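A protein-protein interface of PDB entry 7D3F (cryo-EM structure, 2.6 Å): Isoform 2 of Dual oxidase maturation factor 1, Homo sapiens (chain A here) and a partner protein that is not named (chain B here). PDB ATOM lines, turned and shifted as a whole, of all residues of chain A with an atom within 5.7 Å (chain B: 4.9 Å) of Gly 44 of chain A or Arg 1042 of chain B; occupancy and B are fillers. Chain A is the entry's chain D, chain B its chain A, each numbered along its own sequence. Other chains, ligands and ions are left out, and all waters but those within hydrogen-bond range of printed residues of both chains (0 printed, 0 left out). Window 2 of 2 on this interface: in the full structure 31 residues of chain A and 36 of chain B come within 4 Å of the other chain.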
ATOM      1  N   VAL A  40     -19.568  25.782  10.992  1.00  0.00           N
ATOM      2  CA  VAL A  40     -19.530  25.141  12.305  1.00  0.00           C
ATOM      3  C   VAL A  40     -20.926  24.701  12.724  1.00  0.00           C
ATOM      4  O   VAL A  40     -21.120  23.579  13.209  1.00  0.00           O
ATOM      5  CB  VAL A  40     -18.896  26.085  13.344  1.00  0.00           C
ATOM      6  CG1 VAL A  40     -19.183  25.597  14.755  1.00  0.00           C
ATOM      7  CG2 VAL A  40     -17.396  26.189  13.117  1.00  0.00           C
ATOM      8  N   ILE A  41     -21.926  25.570  12.533  1.00  0.00           N
ATOM      9  CA  ILE A  41     -23.295  25.221  12.921  1.00  0.00           C
ATOM     10  C   ILE A  41     -24.010  24.371  11.884  1.00  0.00           C
ATOM     11  O   ILE A  41     -25.162  23.979  12.113  1.00  0.00           O
ATOM     12  CB  ILE A  41     -24.149  26.475  13.198  1.00  0.00           C
ATOM     13  CG1 ILE A  41     -24.469  27.208  11.896  1.00  0.00           C
ATOM     14  CG2 ILE A  41     -23.439  27.397  14.177  1.00  0.00           C
ATOM     15  CD1 ILE A  41     -25.400  28.388  12.074  1.00  0.00           C
ATOM     16  N   LEU A  42     -23.372  24.085  10.748  1.00  0.00           N
ATOM     17  CA  LEU A  42     -24.003  23.308   9.680  1.00  0.00           C
ATOM     18  C   LEU A  42     -24.578  21.967  10.128  1.00  0.00           C
ATOM     19  O   LEU A  42     -25.711  21.652   9.732  1.00  0.00           O
ATOM     20  CB  LEU A  42     -22.991  23.120   8.539  1.00  0.00           C
ATOM     21  CG  LEU A  42     -23.491  22.446   7.260  1.00  0.00           C
ATOM     22  CD1 LEU A  42     -24.556  23.297   6.588  1.00  0.00           C
ATOM     23  CD2 LEU A  42     -22.333  22.176   6.312  1.00  0.00           C
ATOM     24  N   PRO A  43     -23.882  21.132  10.910  1.00  0.00           N
ATOM     25  CA  PRO A  43     -24.517  19.884  11.370  1.00  0.00           C
ATOM     26  C   PRO A  43     -25.744  20.113  12.233  1.00  0.00           C
ATOM     27  O   PRO A  43     -26.593  19.217  12.328  1.00  0.00           O
ATOM     28  CB  PRO A  43     -23.398  19.183  12.153  1.00  0.00           C
ATOM     29  CG  PRO A  43     -22.144  19.751  11.601  1.00  0.00           C
ATOM     30  CD  PRO A  43     -22.462  21.184  11.306  1.00  0.00           C
ATOM     31  N   GLY A  44     -25.868  21.282  12.864  1.00  0.00           N
ATOM     32  CA  GLY A  44     -27.078  21.612  13.597  1.00  0.00           C
ATOM     33  C   GLY A  44     -28.282  21.840  12.713  1.00  0.00           C
ATOM     34  O   GLY A  44     -29.417  21.716  13.186  1.00  0.00           O
ATOM     35  N   ILE A  45     -28.065  22.176  11.444  1.00  0.00           N
ATOM     36  CA  ILE A  45     -29.157  22.287  10.482  1.00  0.00           C
ATOM     37  C   ILE A  45     -29.710  20.883  10.252  1.00  0.00           C
ATOM     38  O   ILE A  45     -29.043  20.034   9.654  1.00  0.00           O
ATOM     39  CB  ILE A  45     -28.690  22.926   9.169  1.00  0.00           C
ATOM     40  CG1 ILE A  45     -27.934  24.227   9.445  1.00  0.00           C
ATOM     41  CG2 ILE A  45     -29.873  23.188   8.245  1.00  0.00           C
ATOM     42  CD1 ILE A  45     -28.762  25.281  10.149  1.00  0.00           C
ATOM     43  N   ARG A  46     -30.928  20.636  10.724  1.00  0.00           N
ATOM     44  CA  ARG A  46     -31.493  19.296  10.709  1.00  0.00           C
ATOM     45  C   ARG A  46     -32.064  18.952   9.340  1.00  0.00           C
ATOM     46  O   ARG A  46     -32.493  19.827   8.580  1.00  0.00           O
ATOM     47  CB  ARG A  46     -32.585  19.163  11.772  1.00  0.00           C
ATOM     48  N   PHE B1037     -25.163  17.559  19.967  1.00  0.00           N
ATOM     49  CA  PHE B1037     -24.704  18.772  20.634  1.00  0.00           C
ATOM     50  C   PHE B1037     -24.941  19.999  19.769  1.00  0.00           C
ATOM     51  O   PHE B1037     -25.418  21.029  20.259  1.00  0.00           O
ATOM     52  CB  PHE B1037     -23.223  18.645  20.994  1.00  0.00           C
ATOM     53  CG  PHE B1037     -22.634  19.897  21.585  1.00  0.00           C
ATOM     54  CD1 PHE B1037     -22.804  20.191  22.928  1.00  0.00           C
ATOM     55  CD2 PHE B1037     -21.905  20.776  20.799  1.00  0.00           C
ATOM     56  CE1 PHE B1037     -22.262  21.340  23.475  1.00  0.00           C
ATOM     57  CE2 PHE B1037     -21.362  21.927  21.341  1.00  0.00           C
ATOM     58  CZ  PHE B1037     -21.541  22.208  22.681  1.00  0.00           C
ATOM     59  N   ILE B1038     -24.623  19.910  18.475  1.00  0.00           N
ATOM     60  CA  ILE B1038     -24.813  21.074  17.614  1.00  0.00           C
ATOM     61  C   ILE B1038     -26.297  21.372  17.427  1.00  0.00           C
ATOM     62  O   ILE B1038     -26.720  22.530  17.484  1.00  0.00           O
ATOM     63  CB  ILE B1038     -24.096  20.883  16.268  1.00  0.00           C
ATOM     64  CG1 ILE B1038     -22.642  20.491  16.498  1.00  0.00           C
ATOM     65  CG2 ILE B1038     -24.131  22.174  15.474  1.00  0.00           C
ATOM     66  CD1 ILE B1038     -21.887  20.230  15.229  1.00  0.00           C
ATOM     67  N   GLU B1039     -27.116  20.338  17.217  1.00  0.00           N
ATOM     68  CA  GLU B1039     -28.545  20.559  17.027  1.00  0.00           C
ATOM     69  C   GLU B1039     -29.196  21.136  18.276  1.00  0.00           C
ATOM     70  O   GLU B1039     -30.207  21.840  18.180  1.00  0.00           O
ATOM     71  CB  GLU B1039     -29.225  19.248  16.627  1.00  0.00           C
ATOM     72  CG  GLU B1039     -30.660  19.404  16.141  1.00  0.00           C
ATOM     73  CD  GLU B1039     -31.268  18.089  15.685  1.00  0.00           C
ATOM     74  OE1 GLU B1039     -30.672  17.027  15.964  1.00  0.00           O
ATOM     75  OE2 GLU B1039     -32.341  18.120  15.044  1.00  0.00           O
ATOM     76  N   ASN B1040     -28.635  20.852  19.452  1.00  0.00           N
ATOM     77  CA  ASN B1040     -29.206  21.397  20.678  1.00  0.00           C
ATOM     78  C   ASN B1040     -28.699  22.805  20.976  1.00  0.00           C
ATOM     79  O   ASN B1040     -29.455  23.639  21.487  1.00  0.00           O
ATOM     80  CB  ASN B1040     -28.913  20.465  21.855  1.00  0.00           C
ATOM     81  CG  ASN B1040     -29.967  19.384  22.020  1.00  0.00           C
ATOM     82  OD1 ASN B1040     -30.827  19.200  21.159  1.00  0.00           O
ATOM     83  ND2 ASN B1040     -29.903  18.662  23.134  1.00  0.00           N
ATOM     84  N   TYR B1041     -27.433  23.096  20.671  1.00  0.00           N
ATOM     85  CA  TYR B1041     -26.823  24.359  21.072  1.00  0.00           C
ATOM     86  C   TYR B1041     -26.348  25.184  19.879  1.00  0.00           C
ATOM     87  O   TYR B1041     -25.351  25.900  19.980  1.00  0.00           O
ATOM     88  CB  TYR B1041     -25.664  24.108  22.036  1.00  0.00           C
ATOM     89  CG  TYR B1041     -26.073  23.455  23.338  1.00  0.00           C
ATOM     90  CD1 TYR B1041     -26.076  22.074  23.473  1.00  0.00           C
ATOM     91  CD2 TYR B1041     -26.450  24.221  24.434  1.00  0.00           C
ATOM     92  CE1 TYR B1041     -26.445  21.473  24.660  1.00  0.00           C
ATOM     93  CE2 TYR B1041     -26.820  23.629  25.628  1.00  0.00           C
ATOM     94  CZ  TYR B1041     -26.816  22.254  25.735  1.00  0.00           C
ATOM     95  OH  TYR B1041     -27.183  21.654  26.918  1.00  0.00           O
ATOM     96  N   ARG B1042     -27.033  25.085  18.738  1.00  0.00           N
ATOM     97  CA  ARG B1042     -26.677  25.923  17.597  1.00  0.00           C
ATOM     98  C   ARG B1042     -26.848  27.404  17.913  1.00  0.00           C
ATOM     99  O   ARG B1042     -26.031  28.230  17.492  1.00  0.00           O
ATOM    100  CB  ARG B1042     -27.503  25.525  16.372  1.00  0.00           C
ATOM    101  CG  ARG B1042     -28.998  25.395  16.621  1.00  0.00           C
ATOM    102  CD  ARG B1042     -29.669  24.618  15.495  1.00  0.00           C
ATOM    103  NE  ARG B1042     -29.723  25.374  14.246  1.00  0.00           N
ATOM    104  CZ  ARG B1042     -30.845  25.831  13.699  1.00  0.00           C
ATOM    105  NH1 ARG B1042     -32.012  25.602  14.285  1.00  0.00           N
ATOM    106  NH2 ARG B1042     -30.803  26.510  12.560  1.00  0.00           N
ATOM    107  N   ARG B1043     -27.903  27.762  18.650  1.00  0.00           N
ATOM    108  CA  ARG B1043     -28.084  29.158  19.037  1.00  0.00           C
ATOM    109  C   ARG B1043     -26.935  29.638  19.918  1.00  0.00           C
ATOM    110  O   ARG B1043     -26.404  30.739  19.720  1.00  0.00           O
ATOM    111  CB  ARG B1043     -29.418  29.332  19.760  1.00  0.00           C
ATOM    112  CG  ARG B1043     -30.638  28.930  18.952  1.00  0.00           C
ATOM    113  CD  ARG B1043     -31.891  29.019  19.805  1.00  0.00           C
ATOM    114  NE  ARG B1043     -31.819  28.132  20.962  1.00  0.00           N
ATOM    115  CZ  ARG B1043     -32.646  28.188  22.001  1.00  0.00           C
ATOM    116  NH1 ARG B1043     -33.612  29.096  22.036  1.00  0.00           N
ATOM    117  NH2 ARG B1043     -32.504  27.338  23.009  1.00  0.00           N
ATOM    118  N   HIS B1044     -26.538  28.819  20.898  1.00  0.00           N
ATOM    119  CA  HIS B1044     -25.423  29.181  21.764  1.00  0.00           C
ATOM    120  C   HIS B1044     -24.135  29.319  20.965  1.00  0.00           C
ATOM    121  O   HIS B1044     -23.365  30.265  21.170  1.00  0.00           O
ATOM    122  CB  HIS B1044     -25.249  28.137  22.868  1.00  0.00           C
ATOM    123  CG  HIS B1044     -26.510  27.809  23.604  1.00  0.00           C
ATOM    124  ND1 HIS B1044     -27.527  27.063  23.046  1.00  0.00           N
ATOM    125  CD2 HIS B1044     -26.917  28.118  24.858  1.00  0.00           C
ATOM    126  CE1 HIS B1044     -28.506  26.931  23.922  1.00  0.00           C
ATOM    127  NE2 HIS B1044     -28.161  27.562  25.030  1.00  0.00           N
ATOM    128  N   ILE B1045     -23.889  28.384  20.044  1.00  0.00           N
ATOM    129  CA  ILE B1045     -22.678  28.433  19.231  1.00  0.00           C
ATOM    130  C   ILE B1045     -22.662  29.692  18.380  1.00  0.00           C
ATOM    131  O   ILE B1045     -21.637  30.375  18.282  1.00  0.00           O
ATOM    132  CB  ILE B1045     -22.558  27.162  18.369  1.00  0.00           C
ATOM    133  CG1 ILE B1045     -22.266  25.944  19.247  1.00  0.00           C
ATOM    134  CG2 ILE B1045     -21.473  27.327  17.316  1.00  0.00           C
ATOM    135  CD1 ILE B1045     -22.160  24.647  18.476  1.00  0.00           C
ATOM    136  N   GLY B1046     -23.797  30.033  17.767  1.00  0.00           N
ATOM    137  CA  GLY B1046     -23.853  31.231  16.947  1.00  0.00           C
ATOM    138  C   GLY B1046     -23.631  32.502  17.746  1.00  0.00           C
ATOM    139  O   GLY B1046     -22.878  33.385  17.326  1.00  0.00           O
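Of chain B, only Ile 1038 (3.3 Å), Glu 1039 (3.8 Å) and Arg 1042 (3.7 Å) come within 4 Å of Gly 44 of chain A.
Of the printed residues of chain A, Arg 1042 of chain B touches Gly 44 (3.7 Å) and Ile 45 (3.4 Å).
Printed residues of chain A within 4 Å of Glu 1039 of chain B: Gly 44 and Arg 46.
Of the printed residues of chain B, Pro 43 of chain A touches Ile 1038 (3.6 Å).
Of the printed residues of chain A, Ile 1045 of chain B touches Val 40 and Ile 41.
Printed residues of chain B within 4 Å of Ile 45 of chain A: Arg 1042.
CD1 of Ile 1038 of chain B touches O of Val 40 of chain A, at 3.99 Å.
Val 40 of chain A touches Ile 1045 of chain B.
O of Ile 41 of chain A touches CG2 of Ile 1038 of chain B (3.95 Å).
Ile 41 of chain A touches Ile 1045 of chain B (CG2 to CG2, 3.7 Å).
CD1 of Ile 1038 of chain B touches CB of Pro 43 of chain A, at 3.6 Å.
Gly 44 of chain A touches Ile 1038 of chain B.
N of Glu 1039 of chain B touches CA of Gly 44 of chain A (3.8 Å).
CD of Arg 1042 of chain B touches O of Gly 44 of chain A (3.7 Å).
NH2 of Arg 1042 of chain B touches CD1 of Ile 45 of chain A, 3.4 Å away.
Glu 1039 of chain B touches Arg 46 of chain A.
Of the 10 printed residues of chain B, 4 touch a printed residue of chain A.
Hydrophobic or aromatic side chains of chain B within 4 Å of the printed part of chain A: Ile 1038 and Ile 1045.
Printed residues of chain A that touch a printed residue of chain B: Val 40, Ile 41, Pro 43, Gly 44, Ile 45 and Arg 46.
Hydrophobic or aromatic side chains of chain A that line the printed part of chain B: Val 40, Ile 41, Pro 43 and Ile 45.
Among the printed residues, no Asp or Glu carboxylate lies within 4 Å of a Lys or Arg side-chain nitrogen of the other chain.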
